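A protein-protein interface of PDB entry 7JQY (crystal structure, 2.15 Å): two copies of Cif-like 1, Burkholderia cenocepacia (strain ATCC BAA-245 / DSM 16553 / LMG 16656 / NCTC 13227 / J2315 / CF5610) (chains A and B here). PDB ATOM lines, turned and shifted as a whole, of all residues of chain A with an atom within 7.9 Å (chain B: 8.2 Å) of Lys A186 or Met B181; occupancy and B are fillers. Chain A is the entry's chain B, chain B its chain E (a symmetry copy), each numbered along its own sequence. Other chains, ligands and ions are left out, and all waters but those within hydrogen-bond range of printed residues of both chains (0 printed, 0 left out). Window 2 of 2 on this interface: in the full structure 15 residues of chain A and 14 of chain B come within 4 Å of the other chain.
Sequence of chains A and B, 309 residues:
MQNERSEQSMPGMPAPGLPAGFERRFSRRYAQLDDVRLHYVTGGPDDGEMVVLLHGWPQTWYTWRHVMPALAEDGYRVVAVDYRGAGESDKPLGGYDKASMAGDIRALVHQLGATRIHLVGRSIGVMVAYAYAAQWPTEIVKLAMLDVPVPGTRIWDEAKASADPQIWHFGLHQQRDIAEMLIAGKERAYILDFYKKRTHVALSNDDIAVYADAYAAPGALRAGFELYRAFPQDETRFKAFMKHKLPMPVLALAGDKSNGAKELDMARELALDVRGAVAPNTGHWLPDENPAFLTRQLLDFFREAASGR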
ATOM      1  N   GLU A 180      -7.056  22.142  16.004  1.00  0.00           N
ATOM      2  CA  GLU A 180      -5.656  21.799  15.760  1.00  0.00           C
ATOM      3  C   GLU A 180      -4.749  22.990  16.026  1.00  0.00           C
ATOM      4  O   GLU A 180      -3.694  22.853  16.652  1.00  0.00           O
ATOM      5  CB  GLU A 180      -5.479  21.294  14.321  1.00  0.00           C
ATOM      6  CG  GLU A 180      -6.135  19.943  14.072  1.00  0.00           C
ATOM      7  CD  GLU A 180      -7.581  20.054  13.599  1.00  0.00           C
ATOM      8  OE1 GLU A 180      -8.283  21.005  14.022  1.00  0.00           O
ATOM      9  OE2 GLU A 180      -8.030  19.179  12.819  1.00  0.00           O
ATOM     10  N   MET A 181      -5.158  24.175  15.584  1.00  0.00           N
ATOM     11  CA  MET A 181      -4.325  25.351  15.776  1.00  0.00           C
ATOM     12  C   MET A 181      -4.189  25.705  17.254  1.00  0.00           C
ATOM     13  O   MET A 181      -3.131  26.171  17.692  1.00  0.00           O
ATOM     14  CB  MET A 181      -4.909  26.510  14.979  1.00  0.00           C
ATOM     15  CG  MET A 181      -4.571  27.878  15.501  1.00  0.00           C
ATOM     16  SD  MET A 181      -5.691  29.034  14.733  1.00  0.00           S
ATOM     17  CE  MET A 181      -6.770  29.457  16.135  1.00  0.00           C
ATOM     18  N   LEU A 182      -5.258  25.526  18.035  1.00  0.00           N
ATOM     19  CA  LEU A 182      -5.182  25.872  19.453  1.00  0.00           C
ATOM     20  C   LEU A 182      -4.358  24.859  20.233  1.00  0.00           C
ATOM     21  O   LEU A 182      -3.579  25.233  21.116  1.00  0.00           O
ATOM     22  CB  LEU A 182      -6.588  25.962  20.055  1.00  0.00           C
ATOM     23  CG  LEU A 182      -7.492  27.100  19.595  1.00  0.00           C
ATOM     24  CD1 LEU A 182      -8.803  27.031  20.364  1.00  0.00           C
ATOM     25  CD2 LEU A 182      -6.812  28.437  19.794  1.00  0.00           C
ATOM     26  N   ILE A 183      -4.522  23.569  19.932  1.00  0.00           N
ATOM     27  CA  ILE A 183      -3.941  22.534  20.781  1.00  0.00           C
ATOM     28  C   ILE A 183      -2.561  22.046  20.302  1.00  0.00           C
ATOM     29  O   ILE A 183      -1.800  21.489  21.108  1.00  0.00           O
ATOM     30  CB  ILE A 183      -4.957  21.380  20.921  1.00  0.00           C
ATOM     31  CG1 ILE A 183      -6.257  21.910  21.548  1.00  0.00           C
ATOM     32  CG2 ILE A 183      -4.404  20.258  21.793  1.00  0.00           C
ATOM     33  CD1 ILE A 183      -7.443  20.983  21.415  1.00  0.00           C
ATOM     34  N   ALA A 184      -2.195  22.278  19.037  1.00  0.00           N
ATOM     35  CA  ALA A 184      -0.866  21.877  18.564  1.00  0.00           C
ATOM     36  C   ALA A 184       0.227  22.523  19.412  1.00  0.00           C
ATOM     37  O   ALA A 184       0.202  23.734  19.660  1.00  0.00           O
ATOM     38  CB  ALA A 184      -0.682  22.259  17.093  1.00  0.00           C
ATOM     39  N   GLY A 185       1.183  21.707  19.873  1.00  0.00           N
ATOM     40  CA  GLY A 185       2.221  22.176  20.782  1.00  0.00           C
ATOM     41  C   GLY A 185       1.846  22.182  22.253  1.00  0.00           C
ATOM     42  O   GLY A 185       2.715  22.429  23.105  1.00  0.00           O
ATOM     43  N   LYS A 186       0.582  21.941  22.586  1.00  0.00           N
ATOM     44  CA  LYS A 186       0.136  21.877  23.969  1.00  0.00           C
ATOM     45  C   LYS A 186      -0.604  20.576  24.234  1.00  0.00           C
ATOM     46  O   LYS A 186      -1.501  20.523  25.084  1.00  0.00           O
ATOM     47  CB  LYS A 186      -0.728  23.090  24.302  1.00  0.00           C
ATOM     48  CG  LYS A 186       0.058  24.371  24.174  1.00  0.00           C
ATOM     49  CD  LYS A 186      -0.777  25.588  24.359  1.00  0.00           C
ATOM     50  CE  LYS A 186      -0.083  26.793  23.764  1.00  0.00           C
ATOM     51  NZ  LYS A 186      -1.013  27.533  22.882  1.00  0.00           N
ATOM     52  N   GLU A 187      -0.242  19.516  23.502  1.00  0.00           N
ATOM     53  CA  GLU A 187      -0.948  18.249  23.638  1.00  0.00           C
ATOM     54  C   GLU A 187      -0.810  17.705  25.052  1.00  0.00           C
ATOM     55  O   GLU A 187      -1.790  17.225  25.642  1.00  0.00           O
ATOM     56  CB  GLU A 187      -0.431  17.245  22.610  1.00  0.00           C
ATOM     57  CG  GLU A 187      -0.489  17.740  21.160  1.00  0.00           C
ATOM     58  CD  GLU A 187       0.705  18.600  20.771  1.00  0.00           C
ATOM     59  OE1 GLU A 187       1.586  18.843  21.628  1.00  0.00           O
ATOM     60  OE2 GLU A 187       0.751  19.045  19.602  1.00  0.00           O
ATOM     61  N   ARG A 188       0.384  17.818  25.631  1.00  0.00           N
ATOM     62  CA  ARG A 188       0.608  17.295  26.977  1.00  0.00           C
ATOM     63  C   ARG A 188      -0.249  18.021  28.015  1.00  0.00           C
ATOM     64  O   ARG A 188      -0.929  17.389  28.833  1.00  0.00           O
ATOM     65  CB  ARG A 188       2.088  17.416  27.331  1.00  0.00           C
ATOM     66  CG  ARG A 188       2.621  16.271  28.155  1.00  0.00           C
ATOM     67  CD  ARG A 188       4.135  16.333  28.245  1.00  0.00           C
ATOM     68  NE  ARG A 188       4.784  15.238  27.527  1.00  0.00           N
ATOM     69  CZ  ARG A 188       5.967  14.734  27.873  1.00  0.00           C
ATOM     70  NH1 ARG A 188       6.615  15.229  28.920  1.00  0.00           N
ATOM     71  NH2 ARG A 188       6.505  13.732  27.181  1.00  0.00           N
ATOM     72  N   ALA A 189      -0.229  19.353  27.997  1.00  0.00           N
ATOM     73  CA  ALA A 189      -1.015  20.113  28.964  1.00  0.00           C
ATOM     74  C   ALA A 189      -2.513  19.904  28.748  1.00  0.00           C
ATOM     75  O   ALA A 189      -3.286  19.847  29.713  1.00  0.00           O
ATOM     76  CB  ALA A 189      -0.650  21.593  28.887  1.00  0.00           C
ATOM     77  N   TYR A 190      -2.943  19.821  27.490  1.00  0.00           N
ATOM     78  CA  TYR A 190      -4.359  19.627  27.211  1.00  0.00           C
ATOM     79  C   TYR A 190      -4.821  18.240  27.634  1.00  0.00           C
ATOM     80  O   TYR A 190      -5.865  18.099  28.279  1.00  0.00           O
ATOM     81  CB  TYR A 190      -4.633  19.859  25.723  1.00  0.00           C
ATOM     82  CG  TYR A 190      -6.099  19.751  25.327  1.00  0.00           C
ATOM     83  CD1 TYR A 190      -7.014  20.757  25.663  1.00  0.00           C
ATOM     84  CD2 TYR A 190      -6.563  18.664  24.594  1.00  0.00           C
ATOM     85  CE1 TYR A 190      -8.335  20.674  25.283  1.00  0.00           C
ATOM     86  CE2 TYR A 190      -7.896  18.565  24.211  1.00  0.00           C
ATOM     87  CZ  TYR A 190      -8.778  19.575  24.558  1.00  0.00           C
ATOM     88  OH  TYR A 190     -10.103  19.483  24.183  1.00  0.00           O
ATOM     89  N   ILE A 191      -4.042  17.206  27.310  1.00  0.00           N
ATOM     90  CA  ILE A 191      -4.485  15.833  27.527  1.00  0.00           C
ATOM     91  C   ILE A 191      -4.316  15.414  28.985  1.00  0.00           C
ATOM     92  O   ILE A 191      -5.134  14.654  29.517  1.00  0.00           O
ATOM     93  CB  ILE A 191      -3.742  14.897  26.557  1.00  0.00           C
ATOM     94  CG1 ILE A 191      -4.396  14.971  25.182  1.00  0.00           C
ATOM     95  CG2 ILE A 191      -3.716  13.467  27.058  1.00  0.00           C
ATOM     96  CD1 ILE A 191      -3.426  14.653  24.016  1.00  0.00           C
ATOM     97  N   LEU A 192      -3.248  15.864  29.651  1.00  0.00           N
ATOM     98  CA  LEU A 192      -3.101  15.557  31.072  1.00  0.00           C
ATOM     99  C   LEU A 192      -4.249  16.151  31.876  1.00  0.00           C
ATOM    100  O   LEU A 192      -4.766  15.518  32.805  1.00  0.00           O
ATOM    101  CB  LEU A 192      -1.763  16.079  31.601  1.00  0.00           C
ATOM    102  CG  LEU A 192      -0.620  15.086  31.814  1.00  0.00           C
ATOM    103  CD1 LEU A 192      -0.109  14.541  30.476  1.00  0.00           C
ATOM    104  CD2 LEU A 192       0.498  15.773  32.560  1.00  0.00           C
ATOM    105  N   ASP A 193      -4.649  17.380  31.546  1.00  0.00           N
ATOM    106  CA  ASP A 193      -5.764  17.994  32.252  1.00  0.00           C
ATOM    107  C   ASP A 193      -7.062  17.267  31.944  1.00  0.00           C
ATOM    108  O   ASP A 193      -7.833  16.938  32.854  1.00  0.00           O
ATOM    109  CB  ASP A 193      -5.885  19.468  31.883  1.00  0.00           C
ATOM    110  CG  ASP A 193      -6.839  20.208  32.805  1.00  0.00           C
ATOM    111  OD1 ASP A 193      -6.398  20.614  33.903  1.00  0.00           O
ATOM    112  OD2 ASP A 193      -8.024  20.355  32.439  1.00  0.00           O
ATOM    113  N   ALA A 212      -0.401  11.466  25.461  1.00  0.00           N
ATOM    114  CA  ALA A 212      -0.255  12.830  24.962  1.00  0.00           C
ATOM    115  C   ALA A 212       0.813  12.911  23.873  1.00  0.00           C
ATOM    116  O   ALA A 212       0.638  13.631  22.880  1.00  0.00           O
ATOM    117  CB  ALA A 212       0.057  13.783  26.119  1.00  0.00           C
ATOM    118  N   ALA A 216       0.641  14.214  19.799  1.00  0.00           N
ATOM    119  CA  ALA A 216       1.485  15.283  19.279  1.00  0.00           C
ATOM    120  C   ALA A 216       2.102  14.934  17.926  1.00  0.00           C
ATOM    121  O   ALA A 216       2.628  15.824  17.247  1.00  0.00           O
ATOM    122  CB  ALA A 216       2.595  15.611  20.287  1.00  0.00           C
ATOM    123  N   LEU A 221      -3.561  14.800  15.954  1.00  0.00           N
ATOM    124  CA  LEU A 221      -4.632  15.660  16.453  1.00  0.00           C
ATOM    125  C   LEU A 221      -5.782  15.710  15.460  1.00  0.00           C
ATOM    126  O   LEU A 221      -6.948  15.500  15.828  1.00  0.00           O
ATOM    127  CB  LEU A 221      -4.104  17.072  16.708  1.00  0.00           C
ATOM    128  CG  LEU A 221      -3.302  17.378  17.964  1.00  0.00           C
ATOM    129  CD1 LEU A 221      -2.966  18.860  17.961  1.00  0.00           C
ATOM    130  CD2 LEU A 221      -4.092  17.003  19.241  1.00  0.00           C
ATOM    131  N   LEU B 172     -15.882  25.510  25.738  1.00  0.00           N
ATOM    132  CA  LEU B 172     -14.463  25.850  25.819  1.00  0.00           C
ATOM    133  C   LEU B 172     -14.232  27.067  26.701  1.00  0.00           C
ATOM    134  O   LEU B 172     -13.340  27.068  27.555  1.00  0.00           O
ATOM    135  CB  LEU B 172     -13.891  26.098  24.415  1.00  0.00           C
ATOM    136  CG  LEU B 172     -12.495  26.744  24.356  1.00  0.00           C
ATOM    137  CD1 LEU B 172     -11.446  25.865  25.027  1.00  0.00           C
ATOM    138  CD2 LEU B 172     -12.058  27.086  22.914  1.00  0.00           C
ATOM    139  N   GLN B 175     -13.932  26.503  30.441  1.00  0.00           N
ATOM    140  CA  GLN B 175     -12.822  25.724  30.991  1.00  0.00           C
ATOM    141  C   GLN B 175     -11.783  26.701  31.517  1.00  0.00           C
ATOM    142  O   GLN B 175     -10.948  27.208  30.752  1.00  0.00           O
ATOM    143  CB  GLN B 175     -12.217  24.814  29.922  1.00  0.00           C
ATOM    144  CG  GLN B 175     -13.219  23.894  29.245  1.00  0.00           C
ATOM    145  CD  GLN B 175     -14.115  23.215  30.259  1.00  0.00           C
ATOM    146  OE1 GLN B 175     -13.637  22.458  31.099  1.00  0.00           O
ATOM    147  NE2 GLN B 175     -15.423  23.477  30.183  1.00  0.00           N
ATOM    148  N   ARG B 176     -11.796  26.928  32.835  1.00  0.00           N
ATOM    149  CA  ARG B 176     -10.883  27.890  33.446  1.00  0.00           C
ATOM    150  C   ARG B 176      -9.434  27.456  33.257  1.00  0.00           C
ATOM    151  O   ARG B 176      -9.093  26.293  33.494  1.00  0.00           O
ATOM    152  CB  ARG B 176     -11.197  28.044  34.939  1.00  0.00           C
ATOM    153  CG  ARG B 176     -10.506  29.228  35.611  1.00  0.00           C
ATOM    154  CD  ARG B 176     -11.135  29.551  36.977  1.00  0.00           C
ATOM    155  NE  ARG B 176     -12.398  30.285  36.870  1.00  0.00           N
ATOM    156  CZ  ARG B 176     -13.593  29.778  37.167  1.00  0.00           C
ATOM    157  NH1 ARG B 176     -13.699  28.523  37.594  1.00  0.00           N
ATOM    158  NH2 ARG B 176     -14.689  30.524  37.038  1.00  0.00           N
ATOM    159  N   ASP B 177      -8.586  28.410  32.844  1.00  0.00           N
ATOM    160  CA  ASP B 177      -7.150  28.240  32.605  1.00  0.00           C
ATOM    161  C   ASP B 177      -6.869  27.472  31.319  1.00  0.00           C
ATOM    162  O   ASP B 177      -5.902  27.779  30.612  1.00  0.00           O
ATOM    163  CB  ASP B 177      -6.454  27.549  33.782  1.00  0.00           C
ATOM    164  CG  ASP B 177      -6.798  28.185  35.122  1.00  0.00           C
ATOM    165  OD1 ASP B 177      -7.159  27.439  36.054  1.00  0.00           O
ATOM    166  OD2 ASP B 177      -6.678  29.421  35.250  1.00  0.00           O
ATOM    167  N   ILE B 178      -7.685  26.460  31.015  1.00  0.00           N
ATOM    168  CA  ILE B 178      -7.479  25.697  29.789  1.00  0.00           C
ATOM    169  C   ILE B 178      -7.726  26.578  28.570  1.00  0.00           C
ATOM    170  O   ILE B 178      -6.896  26.649  27.654  1.00  0.00           O
ATOM    171  CB  ILE B 178      -8.381  24.447  29.777  1.00  0.00           C
ATOM    172  CG1 ILE B 178      -7.881  23.414  30.790  1.00  0.00           C
ATOM    173  CG2 ILE B 178      -8.476  23.852  28.379  1.00  0.00           C
ATOM    174  CD1 ILE B 178      -6.459  22.948  30.570  1.00  0.00           C
ATOM    175  N   ALA B 179      -8.845  27.309  28.566  1.00  0.00           N
ATOM    176  CA  ALA B 179      -9.158  28.175  27.432  1.00  0.00           C
ATOM    177  C   ALA B 179      -8.079  29.232  27.237  1.00  0.00           C
ATOM    178  O   ALA B 179      -7.692  29.540  26.103  1.00  0.00           O
ATOM    179  CB  ALA B 179     -10.520  28.841  27.628  1.00  0.00           C
ATOM    180  N   GLU B 180      -7.621  29.831  28.333  1.00  0.00           N
ATOM    181  CA  GLU B 180      -6.589  30.850  28.248  1.00  0.00           C
ATOM    182  C   GLU B 180      -5.284  30.268  27.720  1.00  0.00           C
ATOM    183  O   GLU B 180      -4.593  30.905  26.924  1.00  0.00           O
ATOM    184  CB  GLU B 180      -6.389  31.499  29.614  1.00  0.00           C
ATOM    185  CG  GLU B 180      -7.577  32.359  30.064  1.00  0.00           C
ATOM    186  CD  GLU B 180      -8.471  31.674  31.096  1.00  0.00           C
ATOM    187  OE1 GLU B 180      -8.754  30.461  30.959  1.00  0.00           O
ATOM    188  OE2 GLU B 180      -8.901  32.362  32.046  1.00  0.00           O
ATOM    189  N   MET B 181      -4.922  29.067  28.166  1.00  0.00           N
ATOM    190  CA  MET B 181      -3.668  28.473  27.723  1.00  0.00           C
ATOM    191  C   MET B 181      -3.699  28.173  26.230  1.00  0.00           C
ATOM    192  O   MET B 181      -2.690  28.328  25.539  1.00  0.00           O
ATOM    193  CB  MET B 181      -3.381  27.209  28.533  1.00  0.00           C
ATOM    194  CG  MET B 181      -2.463  26.221  27.841  1.00  0.00           C
ATOM    195  SD  MET B 181      -2.423  24.662  28.731  1.00  0.00           S
ATOM    196  CE  MET B 181      -3.637  23.714  27.794  1.00  0.00           C
ATOM    197  N   LEU B 182      -4.854  27.746  25.716  1.00  0.00           N
ATOM    198  CA  LEU B 182      -4.955  27.407  24.306  1.00  0.00           C
ATOM    199  C   LEU B 182      -4.935  28.652  23.425  1.00  0.00           C
ATOM    200  O   LEU B 182      -4.352  28.633  22.337  1.00  0.00           O
ATOM    201  CB  LEU B 182      -6.223  26.601  24.046  1.00  0.00           C
ATOM    202  CG  LEU B 182      -6.364  25.186  24.606  1.00  0.00           C
ATOM    203  CD1 LEU B 182      -7.595  24.539  23.996  1.00  0.00           C
ATOM    204  CD2 LEU B 182      -5.127  24.341  24.334  1.00  0.00           C
ATOM    205  N   ILE B 183      -5.593  29.732  23.852  1.00  0.00           N
ATOM    206  CA  ILE B 183      -5.815  30.868  22.963  1.00  0.00           C
ATOM    207  C   ILE B 183      -4.777  31.978  23.115  1.00  0.00           C
ATOM    208  O   ILE B 183      -4.581  32.751  22.164  1.00  0.00           O
ATOM    209  CB  ILE B 183      -7.249  31.420  23.147  1.00  0.00           C
ATOM    210  CG1 ILE B 183      -8.266  30.330  22.812  1.00  0.00           C
ATOM    211  CG2 ILE B 183      -7.523  32.614  22.230  1.00  0.00           C
ATOM    212  CD1 ILE B 183      -9.617  30.510  23.504  1.00  0.00           C
ATOM    213  N   ALA B 184      -4.069  32.049  24.244  1.00  0.00           N
ATOM    214  CA  ALA B 184      -3.044  33.073  24.406  1.00  0.00           C
ATOM    215  C   ALA B 184      -2.026  32.976  23.270  1.00  0.00           C
ATOM    216  O   ALA B 184      -1.587  31.880  22.912  1.00  0.00           O
ATOM    217  CB  ALA B 184      -2.343  32.924  25.756  1.00  0.00           C
ATOM    218  N   GLY B 185      -1.707  34.124  22.664  1.00  0.00           N
ATOM    219  CA  GLY B 185      -0.840  34.181  21.508  1.00  0.00           C
ATOM    220  C   GLY B 185      -1.524  33.909  20.188  1.00  0.00           C
ATOM    221  O   GLY B 185      -0.907  34.108  19.134  1.00  0.00           O
ATOM    222  N   LYS B 186      -2.779  33.463  20.201  1.00  0.00           N
ATOM    223  CA  LYS B 186      -3.513  33.199  18.972  1.00  0.00           C
ATOM    224  C   LYS B 186      -4.833  33.957  18.954  1.00  0.00           C
ATOM    225  O   LYS B 186      -5.788  33.543  18.282  1.00  0.00           O
ATOM    226  CB  LYS B 186      -3.758  31.702  18.806  1.00  0.00           C
ATOM    227  CG  LYS B 186      -2.488  30.885  18.880  1.00  0.00           C
ATOM    228  CD  LYS B 186      -2.784  29.411  18.742  1.00  0.00           C
ATOM    229  CE  LYS B 186      -1.703  28.583  19.413  1.00  0.00           C
ATOM    230  NZ  LYS B 186      -2.315  27.841  20.549  1.00  0.00           N
ATOM    231  N   LEU B 221      -8.132  37.946  28.042  1.00  0.00           N
ATOM    232  CA  LEU B 221      -8.721  36.641  27.751  1.00  0.00           C
ATOM    233  C   LEU B 221      -9.444  36.083  28.982  1.00  0.00           C
ATOM    234  O   LEU B 221     -10.599  35.646  28.896  1.00  0.00           O
ATOM    235  CB  LEU B 221      -7.649  35.662  27.267  1.00  0.00           C
ATOM    236  CG  LEU B 221      -7.139  35.665  25.813  1.00  0.00           C
ATOM    237  CD1 LEU B 221      -6.098  34.570  25.642  1.00  0.00           C
ATOM    238  CD2 LEU B 221      -8.262  35.475  24.802  1.00  0.00           C
ATOM    239  N   PHE B 225     -13.491  35.422  29.460  1.00  0.00           N
ATOM    240  CA  PHE B 225     -14.009  34.067  29.629  1.00  0.00           C
ATOM    241  C   PHE B 225     -14.830  33.919  30.911  1.00  0.00           C
ATOM    242  O   PHE B 225     -15.699  33.044  30.985  1.00  0.00           O
ATOM    243  CB  PHE B 225     -12.862  33.062  29.620  1.00  0.00           C
ATOM    244  CG  PHE B 225     -12.160  32.952  28.289  1.00  0.00           C
ATOM    245  CD1 PHE B 225     -12.851  33.170  27.104  1.00  0.00           C
ATOM    246  CD2 PHE B 225     -10.812  32.621  28.221  1.00  0.00           C
ATOM    247  CE1 PHE B 225     -12.205  33.059  25.876  1.00  0.00           C
ATOM    248  CE2 PHE B 225     -10.164  32.510  26.988  1.00  0.00           C
ATOM    249  CZ  PHE B 225     -10.864  32.732  25.828  1.00  0.00           C
ATOM    250  N   ARG B 229     -18.171  31.894  32.265  1.00  0.00           N
ATOM    251  CA  ARG B 229     -18.142  31.015  33.420  1.00  0.00           C
ATOM    252  C   ARG B 229     -19.236  31.365  34.422  1.00  0.00           C
ATOM    253  O   ARG B 229     -19.607  30.514  35.235  1.00  0.00           O
ATOM    254  CB  ARG B 229     -16.749  31.063  34.060  1.00  0.00           C
ATOM    255  CG  ARG B 229     -15.691  30.332  33.218  1.00  0.00           C
ATOM    256  CD  ARG B 229     -14.284  30.915  33.332  1.00  0.00           C
ATOM    257  NE  ARG B 229     -13.453  30.442  32.223  1.00  0.00           N
ATOM    258  CZ  ARG B 229     -12.162  30.723  32.060  1.00  0.00           C
ATOM    259  NH1 ARG B 229     -11.518  31.489  32.941  1.00  0.00           N
ATOM    260  NH2 ARG B 229     -11.517  30.236  31.001  1.00  0.00           N
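Among the printed residues, merely in contact across the chains: Leu A182 with Leu B182 (3.5 Å), Leu A182 with Ile B183 (3.8 Å), Ile A183 with Leu B182 (3.8 Å), Lys A186 with Leu B182 (3.6 Å), Ala A189 with Met B181 (3.5 Å), Tyr A190 with Met B181 (3.97 Å) and Asp A193 with Ile B178 (3.5 Å).
Met A181 touches Lys B186, and with the chains exchanged Lys A186 touches Met B181.
Leu B182 touches its own counterpart, Leu A182.
Leu A182 touches Ile B183, and with the chains exchanged Ile A183 touches Leu B182.
Leu A182 touches Lys B186, and with the chains exchanged Lys A186 touches Leu B182.
Positions printed for both chains: 180, 181, 182, 183, 184, 185, 186 and 221.
Of the 11 pairs that touch across the chains among the printed residues, 8 have their exchanged pair printed and touching as well.
O of Leu B182 lies within hydrogen-bond range of NZ of Lys B186, at 2.8 Å.
The side-chain amino group of Lys A186 lies close to the side-chain amino group of Lys B186 (2.7 Å).
The side-chain amino group of Lys B186 sits close to the backbone carbonyl oxygen of Met A181.
NZ of Lys A186 sits at hydrogen-bond distance from O of Met B181.
NZ of Lys B186 sits at hydrogen-bond distance from O of Leu A182 (3.0 Å).
Of the printed residues of chain B, Ile A183 touches Leu B182.
No residue of chain B comes within 4 Å of Gly A185.
Of chain B, only Met B181 (3.2 Å), Leu B182 (3.6 Å) and Lys B186 (2.7 Å) come within 4 Å of Lys A186.
Of the printed residues of chain B, Tyr A190 touches Met B181.
Of the printed residues of chain B, Asp A193 touches Ile B178.
Met B181 touches just these residues of chain A: Lys A186, Ala A189 and Tyr A190.
Of the printed residues of chain A, Lys B186 touches Met A181, Leu A182 and Lys A186.
The nearest residue of chain B that does not touch Lys A186 is Ala B184 (4.4 Å).
Of the 16 printed residues of chain B, 5 touch a printed residue of chain A.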
